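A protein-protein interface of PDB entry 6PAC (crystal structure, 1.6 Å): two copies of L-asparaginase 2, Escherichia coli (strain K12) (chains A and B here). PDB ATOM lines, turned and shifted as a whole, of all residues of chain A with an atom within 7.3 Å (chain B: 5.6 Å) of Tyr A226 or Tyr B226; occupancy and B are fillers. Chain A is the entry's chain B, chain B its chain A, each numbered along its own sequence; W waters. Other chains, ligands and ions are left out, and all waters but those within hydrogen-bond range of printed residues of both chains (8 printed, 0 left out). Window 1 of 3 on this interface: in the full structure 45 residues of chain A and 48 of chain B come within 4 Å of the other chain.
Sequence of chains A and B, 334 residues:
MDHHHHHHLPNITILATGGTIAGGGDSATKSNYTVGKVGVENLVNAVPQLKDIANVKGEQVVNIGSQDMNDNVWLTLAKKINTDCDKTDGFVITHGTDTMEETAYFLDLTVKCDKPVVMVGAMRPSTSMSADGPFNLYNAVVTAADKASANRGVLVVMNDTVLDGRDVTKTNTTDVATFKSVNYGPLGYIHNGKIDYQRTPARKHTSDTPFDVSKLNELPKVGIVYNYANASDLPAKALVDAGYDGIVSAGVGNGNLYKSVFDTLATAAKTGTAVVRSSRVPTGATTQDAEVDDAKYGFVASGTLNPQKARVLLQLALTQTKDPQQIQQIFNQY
OE1 of Gln A308 sits at hydrogen-bond distance from OH of Tyr B226 (2.6 Å).
The side-chain hydroxyl of Tyr B228 sits at hydrogen-bond distance from the backbone NH of Ile A224 (3.5 Å).
NH1 of Arg B280 lies within salt-bridge range of OE2 of Glu A101 (3.9 Å).
OE2 of Glu A102 lies within salt-bridge range of NH1 of Arg B280 (2.7 Å).
The guanidinium group (NE) of Arg B280 lies close to the side-chain amide nitrogen (NE2) of Gln A308, at 3.5 Å.
The side-chain amide oxygen of Gln B308 lies within hydrogen-bond range of the side-chain hydroxyl of Tyr A226 (2.6 Å).
NE2 of Gln B308 lies close to NE of Arg A280 (3.5 Å).
Ile A224 touches Tyr B226, and with the chains exchanged Tyr A226 touches Ile B224.
Ile A224 touches Tyr B228, and with the chains exchanged Tyr A228 touches Ile B224.
Tyr B226 touches its own counterpart, Tyr A226.
Arg A280 touches Gln B308, and with the chains exchanged Gln A308 touches Arg B280.
Of the 12 pairs that touch across the chains among the printed residues, 9 have their exchanged pair printed and touching as well.
The side-chain amide nitrogen of Asn A306 lies within hydrogen-bond range of the side-chain carboxylate of Glu A101 (3.3 Å).
The backbone carbonyl oxygen (O) of Glu A101 is in hydrogen-bond range of the side-chain amino group (NZ) of Lys A309, at 2.9 Å.
O of Gly A251 sits at hydrogen-bond distance from N of Arg A280 (2.8 Å).
Val A225 touches none of the printed residues of chain B.
Of chain B, only Ile B224 (3.6 Å), Tyr B226 (3.6 Å) and Gln B308 (2.6 Å) come within 4 Å of Tyr A226.
Ser A279 touches none of the printed residues of chain B.
Of the printed residues of chain B, Arg A280 touches Gln B308.
Of the printed residues of chain A, Tyr B226 touches Ile A224 (3.6 Å), Tyr A226 (3.6 Å) and Gln A308 (2.6 Å).
Of the printed residues of chain A, Tyr B228 touches Glu A102 (3.6 Å) and Ile A224 (3.5 Å).
The nearest residue of chain B that does not touch Tyr A226 is Pro B307 (4.02 Å).
The nearest printed residue of chain B that does not touch Arg A280 is Arg B280 (5.7 Å).
Tyr B228 touches Glu A102 (CB to OE1, 3.6 Å).
CG2 of Ile A224 touches CD2 of Tyr B226, at 3.6 Å.
CG2 of Ile B224 touches CD2 of Tyr A226, at 3.6 Å.
Tyr A226 touches Tyr B226 (CD1 to CD1, 3.6 Å).
Ile B224 touches Tyr A228 (N to OH, 3.6 Å).
Of the 12 printed residues of chain B, 5 touch a printed residue of chain A.
Hydrophobic or aromatic side chains of chain B within 4 Å of the printed part of chain A: Ile B224, Tyr B226 and Tyr B228.
Among the printed residues, 12 pairs touch across the chains.
Among the printed residues, Asp or Glu carboxylates within 4 Å of a Lys or Arg side-chain nitrogen of the other chain: Glu A101 with Arg B280 and Glu A102 with Arg B280.
Water W2 lies within hydrogen-bond range of the side-chain hydroxyl (OH) of Tyr B228 and the backbone carbonyl oxygen (O) of Ile A224.
Water W3 lies within hydrogen-bond range of O of Ile B224 and N of Tyr A226.
Water W1 lies within hydrogen-bond range of the side-chain amide nitrogen (NE2) of Gln B308 (3.0 Å), the backbone carbonyl oxygen (O) of Arg A280 (3.1 Å) and the side-chain hydroxyl (OH) of Tyr A226 (3.5 Å).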
ATOM      1  N   GLU A 101     -34.112  16.282  16.759  1.00  0.00           N
ATOM      2  CA  GLU A 101     -33.281  16.089  15.594  1.00  0.00           C
ATOM      3  C   GLU A 101     -31.819  15.761  15.942  1.00  0.00           C
ATOM      4  O   GLU A 101     -31.112  15.267  15.083  1.00  0.00           O
ATOM      5  CB  GLU A 101     -33.323  17.317  14.701  1.00  0.00           C
ATOM      6  CG  GLU A 101     -32.508  18.531  15.225  1.00  0.00           C
ATOM      7  CD  GLU A 101     -32.946  19.861  14.540  1.00  0.00           C
ATOM      8  OE1 GLU A 101     -32.151  20.353  13.684  1.00  0.00           O
ATOM      9  OE2 GLU A 101     -34.071  20.338  14.801  1.00  0.00           O
ATOM     10  N   GLU A 102     -31.368  16.184  17.109  1.00  0.00           N
ATOM     11  CA  GLU A 102     -29.995  15.933  17.529  1.00  0.00           C
ATOM     12  C   GLU A 102     -29.872  14.483  18.016  1.00  0.00           C
ATOM     13  O   GLU A 102     -28.982  13.784  17.551  1.00  0.00           O
ATOM     14  CB  GLU A 102     -29.577  16.964  18.577  1.00  0.00           C
ATOM     15  CG  GLU A 102     -29.611  18.388  18.060  1.00  0.00           C
ATOM     16  CD  GLU A 102     -29.353  19.429  19.163  1.00  0.00           C
ATOM     17  OE1 GLU A 102     -28.335  19.251  19.895  1.00  0.00           O
ATOM     18  OE2 GLU A 102     -30.119  20.426  19.267  1.00  0.00           O
ATOM     19  N   ILE A 224     -20.727  25.438  19.788  1.00  0.00           N
ATOM     20  CA  ILE A 224     -21.201  26.117  18.549  1.00  0.00           C
ATOM     21  C   ILE A 224     -21.157  27.591  18.716  1.00  0.00           C
ATOM     22  O   ILE A 224     -21.630  28.174  19.748  1.00  0.00           O
ATOM     23  CB  ILE A 224     -22.667  25.695  18.206  1.00  0.00           C
ATOM     24  CG1 ILE A 224     -22.742  24.194  18.042  1.00  0.00           C
ATOM     25  CG2 ILE A 224     -23.157  26.469  16.969  1.00  0.00           C
ATOM     26  CD1 ILE A 224     -24.166  23.584  17.778  1.00  0.00           C
ATOM     27  N   VAL A 225     -20.565  28.251  17.717  1.00  0.00           N
ATOM     28  CA  VAL A 225     -20.536  29.694  17.705  1.00  0.00           C
ATOM     29  C   VAL A 225     -21.345  30.220  16.502  1.00  0.00           C
ATOM     30  O   VAL A 225     -21.383  29.621  15.456  1.00  0.00           O
ATOM     31  CB  VAL A 225     -19.079  30.268  17.686  1.00  0.00           C
ATOM     32  CG1 VAL A 225     -18.365  29.836  18.953  1.00  0.00           C
ATOM     33  CG2 VAL A 225     -18.324  29.835  16.454  1.00  0.00           C
ATOM     34  N   TYR A 226     -21.930  31.396  16.670  1.00  0.00           N
ATOM     35  CA  TYR A 226     -22.825  32.006  15.621  1.00  0.00           C
ATOM     36  C   TYR A 226     -22.194  33.164  14.929  1.00  0.00           C
ATOM     37  O   TYR A 226     -21.497  33.926  15.584  1.00  0.00           O
ATOM     38  CB  TYR A 226     -24.104  32.453  16.318  1.00  0.00           C
ATOM     39  CG  TYR A 226     -25.334  32.489  15.451  1.00  0.00           C
ATOM     40  CD1 TYR A 226     -25.981  31.326  15.113  1.00  0.00           C
ATOM     41  CD2 TYR A 226     -25.888  33.687  15.000  1.00  0.00           C
ATOM     42  CE1 TYR A 226     -27.130  31.352  14.309  1.00  0.00           C
ATOM     43  CE2 TYR A 226     -27.029  33.721  14.259  1.00  0.00           C
ATOM     44  CZ  TYR A 226     -27.694  32.543  13.934  1.00  0.00           C
ATOM     45  OH  TYR A 226     -28.828  32.498  13.127  1.00  0.00           O
ATOM     46  N   ASN A 227     -22.418  33.269  13.613  1.00  0.00           N
ATOM     47  CA  ASN A 227     -21.864  34.384  12.814  1.00  0.00           C
ATOM     48  C   ASN A 227     -22.988  35.274  12.380  1.00  0.00           C
ATOM     49  O   ASN A 227     -24.128  34.783  12.166  1.00  0.00           O
ATOM     50  CB  ASN A 227     -21.075  33.874  11.604  1.00  0.00           C
ATOM     51  CG  ASN A 227     -19.770  33.178  11.995  1.00  0.00           C
ATOM     52  OD1 ASN A 227     -18.743  33.799  11.959  1.00  0.00           O
ATOM     53  ND2 ASN A 227     -19.846  31.890  12.380  1.00  0.00           N
ATOM     54  N   TYR A 228     -22.669  36.563  12.275  1.00  0.00           N
ATOM     55  CA  TYR A 228     -23.665  37.607  11.991  1.00  0.00           C
ATOM     56  C   TYR A 228     -22.773  38.849  11.780  1.00  0.00           C
ATOM     57  O   TYR A 228     -21.537  38.780  11.975  1.00  0.00           O
ATOM     58  CB  TYR A 228     -24.715  37.773  13.127  1.00  0.00           C
ATOM     59  CG  TYR A 228     -24.062  37.971  14.471  1.00  0.00           C
ATOM     60  CD1 TYR A 228     -23.605  36.861  15.176  1.00  0.00           C
ATOM     61  CD2 TYR A 228     -23.868  39.212  14.968  1.00  0.00           C
ATOM     62  CE1 TYR A 228     -23.009  37.015  16.429  1.00  0.00           C
ATOM     63  CE2 TYR A 228     -23.273  39.403  16.223  1.00  0.00           C
ATOM     64  CZ  TYR A 228     -22.856  38.296  16.931  1.00  0.00           C
ATOM     65  OH  TYR A 228     -22.225  38.584  18.121  1.00  0.00           O
ATOM     66  N   ALA A 231     -19.895  40.285  14.370  1.00  0.00           N
ATOM     67  CA  ALA A 231     -19.848  39.244  15.411  1.00  0.00           C
ATOM     68  C   ALA A 231     -18.686  39.334  16.338  1.00  0.00           C
ATOM     69  O   ALA A 231     -17.582  39.621  15.900  1.00  0.00           O
ATOM     70  CB  ALA A 231     -19.846  37.885  14.762  1.00  0.00           C
ATOM     71  N   SER A 232     -18.937  39.062  17.596  1.00  0.00           N
ATOM     72  CA  SER A 232     -17.870  38.992  18.575  1.00  0.00           C
ATOM     73  C   SER A 232     -17.080  37.712  18.443  1.00  0.00           C
ATOM     74  O   SER A 232     -17.645  36.627  18.224  1.00  0.00           O
ATOM     75  CB  SER A 232     -18.449  39.057  20.009  1.00  0.00           C
ATOM     76  OG  SER A 232     -17.375  39.004  20.944  1.00  0.00           O
ATOM     77  N   PRO A 235     -17.249  34.467  22.213  1.00  0.00           N
ATOM     78  CA  PRO A 235     -17.679  33.061  22.347  1.00  0.00           C
ATOM     79  C   PRO A 235     -16.618  32.055  21.867  1.00  0.00           C
ATOM     80  O   PRO A 235     -16.330  31.050  22.586  1.00  0.00           O
ATOM     81  CB  PRO A 235     -18.956  33.016  21.490  1.00  0.00           C
ATOM     82  CG  PRO A 235     -19.530  34.445  21.662  1.00  0.00           C
ATOM     83  CD  PRO A 235     -18.303  35.297  21.587  1.00  0.00           C
ATOM     84  N   ALA A 236     -16.106  32.242  20.641  1.00  0.00           N
ATOM     85  CA  ALA A 236     -15.064  31.344  20.104  1.00  0.00           C
ATOM     86  C   ALA A 236     -13.826  31.267  21.039  1.00  0.00           C
ATOM     87  O   ALA A 236     -13.316  30.175  21.406  1.00  0.00           O
ATOM     88  CB  ALA A 236     -14.697  31.767  18.710  1.00  0.00           C
ATOM     89  N   VAL A 248     -17.930  23.967  16.212  1.00  0.00           N
ATOM     90  CA  VAL A 248     -18.722  24.085  14.999  1.00  0.00           C
ATOM     91  C   VAL A 248     -19.099  25.565  14.866  1.00  0.00           C
ATOM     92  O   VAL A 248     -19.632  26.178  15.800  1.00  0.00           O
ATOM     93  CB  VAL A 248     -19.998  23.216  15.030  1.00  0.00           C
ATOM     94  CG1 VAL A 248     -20.855  23.415  13.770  1.00  0.00           C
ATOM     95  CG2 VAL A 248     -19.658  21.747  15.170  1.00  0.00           C
ATOM     96  N   SER A 249     -18.859  26.105  13.676  1.00  0.00           N
ATOM     97  CA  SER A 249     -19.278  27.426  13.314  1.00  0.00           C
ATOM     98  C   SER A 249     -20.641  27.407  12.610  1.00  0.00           C
ATOM     99  O   SER A 249     -20.738  26.833  11.558  1.00  0.00           O
ATOM    100  CB  SER A 249     -18.237  28.062  12.416  1.00  0.00           C
ATOM    101  OG  SER A 249     -18.723  29.268  11.876  1.00  0.00           O
ATOM    102  N   ALA A 250     -21.618  28.144  13.151  1.00  0.00           N
ATOM    103  CA  ALA A 250     -22.834  28.417  12.423  1.00  0.00           C
ATOM    104  C   ALA A 250     -22.548  29.662  11.577  1.00  0.00           C
ATOM    105  O   ALA A 250     -22.743  30.793  12.005  1.00  0.00           O
ATOM    106  CB  ALA A 250     -23.991  28.613  13.362  1.00  0.00           C
ATOM    107  N   GLY A 251     -21.984  29.413  10.414  1.00  0.00           N
ATOM    108  CA  GLY A 251     -21.560  30.443   9.495  1.00  0.00           C
ATOM    109  C   GLY A 251     -22.689  31.204   8.811  1.00  0.00           C
ATOM    110  O   GLY A 251     -23.861  30.845   8.924  1.00  0.00           O
ATOM    111  N   VAL A 252     -22.323  32.278   8.125  1.00  0.00           N
ATOM    112  CA  VAL A 252     -23.270  32.984   7.311  1.00  0.00           C
ATOM    113  C   VAL A 252     -23.144  32.411   5.887  1.00  0.00           C
ATOM    114  O   VAL A 252     -22.062  32.069   5.425  1.00  0.00           O
ATOM    115  CB  VAL A 252     -23.069  34.516   7.414  1.00  0.00           C
ATOM    116  CG1 VAL A 252     -23.310  34.952   8.839  1.00  0.00           C
ATOM    117  CG2 VAL A 252     -21.688  35.000   6.956  1.00  0.00           C
ATOM    118  N   TYR A 258     -17.285  35.657  10.087  1.00  0.00           N
ATOM    119  CA  TYR A 258     -16.902  37.022  10.344  1.00  0.00           C
ATOM    120  C   TYR A 258     -15.413  37.076  10.646  1.00  0.00           C
ATOM    121  O   TYR A 258     -14.882  36.171  11.294  1.00  0.00           O
ATOM    122  CB  TYR A 258     -17.741  37.614  11.534  1.00  0.00           C
ATOM    123  CG  TYR A 258     -17.401  39.022  11.791  1.00  0.00           C
ATOM    124  CD1 TYR A 258     -17.909  40.006  11.009  1.00  0.00           C
ATOM    125  CD2 TYR A 258     -16.608  39.400  12.858  1.00  0.00           C
ATOM    126  CE1 TYR A 258     -17.622  41.348  11.214  1.00  0.00           C
ATOM    127  CE2 TYR A 258     -16.308  40.729  13.088  1.00  0.00           C
ATOM    128  CZ  TYR A 258     -16.831  41.697  12.293  1.00  0.00           C
ATOM    129  OH  TYR A 258     -16.590  43.044  12.473  1.00  0.00           O
ATOM    130  N   VAL A 261     -13.976  36.065  14.079  1.00  0.00           N
ATOM    131  CA  VAL A 261     -14.269  34.654  14.336  1.00  0.00           C
ATOM    132  C   VAL A 261     -13.342  33.777  13.493  1.00  0.00           C
ATOM    133  O   VAL A 261     -12.762  32.828  13.967  1.00  0.00           O
ATOM    134  CB  VAL A 261     -15.803  34.343  14.119  1.00  0.00           C
ATOM    135  CG1 VAL A 261     -16.116  32.883  14.295  1.00  0.00           C
ATOM    136  CG2 VAL A 261     -16.635  35.232  15.002  1.00  0.00           C
ATOM    137  N   SER A 279     -23.464  26.126   8.773  1.00  0.00           N
ATOM    138  CA  SER A 279     -24.169  27.324   8.378  1.00  0.00           C
ATOM    139  C   SER A 279     -25.450  27.509   9.217  1.00  0.00           C
ATOM    140  O   SER A 279     -26.156  26.525   9.465  1.00  0.00           O
ATOM    141  CB  SER A 279     -24.605  27.291   6.896  1.00  0.00           C
ATOM    142  OG  SER A 279     -25.212  28.569   6.586  1.00  0.00           O
ATOM    143  N   ARG A 280     -25.732  28.791   9.547  1.00  0.00           N
ATOM    144  CA  ARG A 280     -26.990  29.206  10.134  1.00  0.00           C
ATOM    145  C   ARG A 280     -28.135  29.123   9.125  1.00  0.00           C
ATOM    146  O   ARG A 280     -29.292  29.188   9.523  1.00  0.00           O
ATOM    147  CB  ARG A 280     -26.895  30.627  10.711  1.00  0.00           C
ATOM    148  CG  ARG A 280     -26.987  31.700   9.663  1.00  0.00           C
ATOM    149  CD  ARG A 280     -26.685  33.060  10.230  1.00  0.00           C
ATOM    150  NE  ARG A 280     -26.989  34.070   9.211  1.00  0.00           N
ATOM    151  CZ  ARG A 280     -26.860  35.374   9.424  1.00  0.00           C
ATOM    152  NH1 ARG A 280     -27.293  36.232   8.492  1.00  0.00           N
ATOM    153  NH2 ARG A 280     -26.428  35.850  10.563  1.00  0.00           N
ATOM    154  N   VAL A 281     -27.809  28.988   7.855  1.00  0.00           N
ATOM    155  CA  VAL A 281     -28.823  28.936   6.827  1.00  0.00           C
ATOM    156  C   VAL A 281     -29.517  27.566   6.910  1.00  0.00           C
ATOM    157  O   VAL A 281     -28.831  26.561   6.951  1.00  0.00           O
ATOM    158  CB  VAL A 281     -28.133  29.239   5.478  1.00  0.00           C
ATOM    159  CG1 VAL A 281     -29.067  29.078   4.322  1.00  0.00           C
ATOM    160  CG2 VAL A 281     -27.586  30.674   5.458  1.00  0.00           C
ATOM    161  N   ASN A 306     -26.430  20.763   9.603  1.00  0.00           N
ATOM    162  CA  ASN A 306     -26.609  22.036  10.271  1.00  0.00           C
ATOM    163  C   ASN A 306     -25.764  22.040  11.536  1.00  0.00           C
ATOM    164  O   ASN A 306     -25.133  21.053  11.844  1.00  0.00           O
ATOM    165  CB  ASN A 306     -28.115  22.357  10.448  1.00  0.00           C
ATOM    166  CG  ASN A 306     -28.815  21.503  11.500  1.00  0.00           C
ATOM    167  OD1 ASN A 306     -28.208  21.073  12.477  1.00  0.00           O
ATOM    168  ND2 ASN A 306     -30.107  21.245  11.288  1.00  0.00           N
ATOM    169  N   PRO A 307     -25.687  23.167  12.238  1.00  0.00           N
ATOM    170  CA  PRO A 307     -24.642  23.267  13.313  1.00  0.00           C
ATOM    171  C   PRO A 307     -24.803  22.205  14.395  1.00  0.00           C
ATOM    172  O   PRO A 307     -23.825  21.554  14.785  1.00  0.00           O
ATOM    173  CB  PRO A 307     -24.843  24.702  13.852  1.00  0.00           C
ATOM    174  CG  PRO A 307     -25.365  25.441  12.625  1.00  0.00           C
ATOM    175  CD  PRO A 307     -26.303  24.467  11.948  1.00  0.00           C
ATOM    176  N   GLN A 308     -26.030  21.984  14.816  1.00  0.00           N
ATOM    177  CA  GLN A 308     -26.274  21.022  15.893  1.00  0.00           C
ATOM    178  C   GLN A 308     -26.097  19.587  15.412  1.00  0.00           C
ATOM    179  O   GLN A 308     -25.676  18.725  16.203  1.00  0.00           O
ATOM    180  CB  GLN A 308     -27.625  21.297  16.541  1.00  0.00           C
ATOM    181  CG  GLN A 308     -28.873  21.195  15.618  1.00  0.00           C
ATOM    182  CD  GLN A 308     -29.257  22.537  15.022  1.00  0.00           C
ATOM    183  OE1 GLN A 308     -28.422  23.477  14.960  1.00  0.00           O
ATOM    184  NE2 GLN A 308     -30.527  22.610  14.484  1.00  0.00           N
ATOM    185  N   LYS A 309     -26.392  19.328  14.158  1.00  0.00           N
ATOM    186  CA  LYS A 309     -26.117  17.984  13.590  1.00  0.00           C
ATOM    187  C   LYS A 309     -24.643  17.776  13.373  1.00  0.00           C
ATOM    188  O   LYS A 309     -24.058  16.705  13.594  1.00  0.00           O
ATOM    189  CB  LYS A 309     -26.728  17.859  12.216  1.00  0.00           C
ATOM    190  CG  LYS A 309     -28.222  17.955  12.182  1.00  0.00           C
ATOM    191  CD  LYS A 309     -28.959  16.654  12.312  1.00  0.00           C
ATOM    192  CE  LYS A 309     -30.458  16.815  11.971  1.00  0.00           C
ATOM    193  NZ  LYS A 309     -31.202  15.559  12.224  1.00  0.00           N
ATOM    194  N   ILE B 224     -24.884  37.107  20.075  1.00  0.00           N
ATOM    195  CA  ILE B 224     -25.776  35.988  19.903  1.00  0.00           C
ATOM    196  C   ILE B 224     -25.194  34.686  20.422  1.00  0.00           C
ATOM    197  O   ILE B 224     -24.059  34.348  20.118  1.00  0.00           O
ATOM    198  CB  ILE B 224     -26.156  35.803  18.404  1.00  0.00           C
ATOM    199  CG1 ILE B 224     -26.746  37.094  17.792  1.00  0.00           C
ATOM    200  CG2 ILE B 224     -27.133  34.642  18.248  1.00  0.00           C
ATOM    201  CD1 ILE B 224     -27.130  37.116  16.324  1.00  0.00           C
ATOM    202  N   VAL B 225     -25.997  33.969  21.223  1.00  0.00           N
ATOM    203  CA  VAL B 225     -25.623  32.670  21.744  1.00  0.00           C
ATOM    204  C   VAL B 225     -26.523  31.579  21.146  1.00  0.00           C
ATOM    205  O   VAL B 225     -27.702  31.830  20.988  1.00  0.00           O
ATOM    206  CB  VAL B 225     -25.637  32.653  23.303  1.00  0.00           C
ATOM    207  CG1 VAL B 225     -24.568  33.671  23.811  1.00  0.00           C
ATOM    208  CG2 VAL B 225     -26.997  32.937  23.921  1.00  0.00           C
ATOM    209  N   TYR B 226     -25.955  30.419  20.890  1.00  0.00           N
ATOM    210  CA  TYR B 226     -26.707  29.291  20.294  1.00  0.00           C
ATOM    211  C   TYR B 226     -27.071  28.213  21.387  1.00  0.00           C
ATOM    212  O   TYR B 226     -26.257  27.863  22.280  1.00  0.00           O
ATOM    213  CB  TYR B 226     -25.831  28.667  19.211  1.00  0.00           C
ATOM    214  CG  TYR B 226     -26.581  27.955  18.119  1.00  0.00           C
ATOM    215  CD1 TYR B 226     -27.285  28.702  17.156  1.00  0.00           C
ATOM    216  CD2 TYR B 226     -26.579  26.557  18.004  1.00  0.00           C
ATOM    217  CE1 TYR B 226     -27.920  28.091  16.145  1.00  0.00           C
ATOM    218  CE2 TYR B 226     -27.231  25.931  16.996  1.00  0.00           C
ATOM    219  CZ  TYR B 226     -27.900  26.677  16.015  1.00  0.00           C
ATOM    220  OH  TYR B 226     -28.582  26.109  14.934  1.00  0.00           O
ATOM    221  N   ASN B 227     -28.292  27.689  21.325  1.00  0.00           N
ATOM    222  CA  ASN B 227     -28.687  26.527  22.137  1.00  0.00           C
ATOM    223  C   ASN B 227     -28.796  25.244  21.348  1.00  0.00           C
ATOM    224  O   ASN B 227     -29.105  25.230  20.149  1.00  0.00           O
ATOM    225  CB  ASN B 227     -30.016  26.802  22.822  1.00  0.00           C
ATOM    226  CG  ASN B 227     -29.915  27.941  23.824  1.00  0.00           C
ATOM    227  OD1 ASN B 227     -29.821  27.687  25.035  1.00  0.00           O
ATOM    228  ND2 ASN B 227     -29.999  29.216  23.336  1.00  0.00           N
ATOM    229  N   TYR B 228     -28.498  24.155  22.047  1.00  0.00           N
ATOM    230  CA  TYR B 228     -28.426  22.787  21.447  1.00  0.00           C
ATOM    231  C   TYR B 228     -28.293  21.863  22.674  1.00  0.00           C
ATOM    232  O   TYR B 228     -28.209  22.357  23.787  1.00  0.00           O
ATOM    233  CB  TYR B 228     -27.261  22.662  20.475  1.00  0.00           C
ATOM    234  CG  TYR B 228     -25.901  23.128  21.042  1.00  0.00           C
ATOM    235  CD1 TYR B 228     -25.571  24.469  21.113  1.00  0.00           C
ATOM    236  CD2 TYR B 228     -25.014  22.203  21.538  1.00  0.00           C
ATOM    237  CE1 TYR B 228     -24.378  24.878  21.642  1.00  0.00           C
ATOM    238  CE2 TYR B 228     -23.791  22.605  22.050  1.00  0.00           C
ATOM    239  CZ  TYR B 228     -23.505  23.941  22.117  1.00  0.00           C
ATOM    240  OH  TYR B 228     -22.338  24.416  22.673  1.00  0.00           O
ATOM    241  N   ALA B 231     -25.497  22.270  25.753  1.00  0.00           N
ATOM    242  CA  ALA B 231     -24.928  23.580  25.387  1.00  0.00           C
ATOM    243  C   ALA B 231     -23.994  24.107  26.461  1.00  0.00           C
ATOM    244  O   ALA B 231     -24.296  24.016  27.648  1.00  0.00           O
ATOM    245  CB  ALA B 231     -25.996  24.589  25.122  1.00  0.00           C
ATOM    246  N   SER B 232     -22.939  24.775  26.044  1.00  0.00           N
ATOM    247  CA  SER B 232     -22.029  25.471  26.985  1.00  0.00           C
ATOM    248  C   SER B 232     -22.580  26.809  27.391  1.00  0.00           C
ATOM    249  O   SER B 232     -23.155  27.554  26.530  1.00  0.00           O
ATOM    250  CB  SER B 232     -20.686  25.758  26.302  1.00  0.00           C
ATOM    251  OG  SER B 232     -19.767  26.341  27.231  1.00  0.00           O
ATOM    252  N   ALA B 250     -30.350  32.282  20.436  1.00  0.00           N
ATOM    253  CA  ALA B 250     -30.910  31.391  19.403  1.00  0.00           C
ATOM    254  C   ALA B 250     -31.379  30.146  20.074  1.00  0.00           C
ATOM    255  O   ALA B 250     -30.608  29.212  20.225  1.00  0.00           O
ATOM    256  CB  ALA B 250     -29.897  31.065  18.322  1.00  0.00           C
ATOM    257  N   VAL B 261     -27.393  27.942  30.189  1.00  0.00           N
ATOM    258  CA  VAL B 261     -27.515  29.208  29.416  1.00  0.00           C
ATOM    259  C   VAL B 261     -28.591  30.086  30.037  1.00  0.00           C
ATOM    260  O   VAL B 261     -28.397  31.246  30.217  1.00  0.00           O
ATOM    261  CB  VAL B 261     -27.753  28.882  27.924  1.00  0.00           C
ATOM    262  CG1 VAL B 261     -27.939  30.204  27.133  1.00  0.00           C
ATOM    263  CG2 VAL B 261     -26.614  28.077  27.332  1.00  0.00           C
ATOM    264  N   ARG B 280     -33.285  29.311  16.918  1.00  0.00           N
ATOM    265  CA  ARG B 280     -32.560  28.744  15.838  1.00  0.00           C
ATOM    266  C   ARG B 280     -33.441  28.135  14.765  1.00  0.00           C
ATOM    267  O   ARG B 280     -32.988  27.864  13.654  1.00  0.00           O
ATOM    268  CB  ARG B 280     -31.598  27.677  16.308  1.00  0.00           C
ATOM    269  CG  ARG B 280     -32.308  26.349  16.646  1.00  0.00           C
ATOM    270  CD  ARG B 280     -31.336  25.366  17.243  1.00  0.00           C
ATOM    271  NE  ARG B 280     -31.938  24.030  17.328  1.00  0.00           N
ATOM    272  CZ  ARG B 280     -31.316  22.952  17.817  1.00  0.00           C
ATOM    273  NH1 ARG B 280     -31.924  21.746  17.750  1.00  0.00           N
ATOM    274  NH2 ARG B 280     -30.136  23.075  18.432  1.00  0.00           N
ATOM    275  N   PRO B 307     -32.462  35.194  14.958  1.00  0.00           N
ATOM    276  CA  PRO B 307     -31.540  35.815  15.947  1.00  0.00           C
ATOM    277  C   PRO B 307     -30.800  37.030  15.450  1.00  0.00           C
ATOM    278  O   PRO B 307     -30.668  38.031  16.165  1.00  0.00           O
ATOM    279  CB  PRO B 307     -30.615  34.672  16.282  1.00  0.00           C
ATOM    280  CG  PRO B 307     -31.492  33.438  16.120  1.00  0.00           C
ATOM    281  CD  PRO B 307     -32.228  33.758  14.864  1.00  0.00           C
ATOM    282  N   GLN B 308     -30.336  36.959  14.191  1.00  0.00           N
ATOM    283  CA  GLN B 308     -29.614  38.093  13.640  1.00  0.00           C
ATOM    284  C   GLN B 308     -30.482  39.312  13.380  1.00  0.00           C
ATOM    285  O   GLN B 308     -29.995  40.448  13.513  1.00  0.00           O
ATOM    286  CB  GLN B 308     -28.829  37.667  12.368  1.00  0.00           C
ATOM    287  CG  GLN B 308     -29.611  37.039  11.225  1.00  0.00           C
ATOM    288  CD  GLN B 308     -29.839  35.514  11.338  1.00  0.00           C
ATOM    289  OE1 GLN B 308     -29.584  34.919  12.409  1.00  0.00           O
ATOM    290  NE2 GLN B 308     -30.211  34.850  10.230  1.00  0.00           N
HETATM  291  O   HOH W   1     -30.588  31.911  10.175  1.00  0.00           O
HETATM  292  O   HOH W   2     -21.560  26.803  22.795  1.00  0.00           O
HETATM  293  O   HOH W   3     -22.137  32.500  19.472  1.00  0.00           O
HETATM  294  O   HOH W   4     -31.530  25.163  13.225  1.00  0.00           O
HETATM  295  O   HOH W   5     -28.659  27.508  12.482  1.00  0.00           O
HETATM  296  O   HOH W   6     -31.963  28.203  10.712  1.00  0.00           O
HETATM  297  O   HOH W   7     -34.047  22.900  15.534  1.00  0.00           O
HETATM  298  O   HOH W   8     -22.783  30.258  20.919  1.00  0.00           O
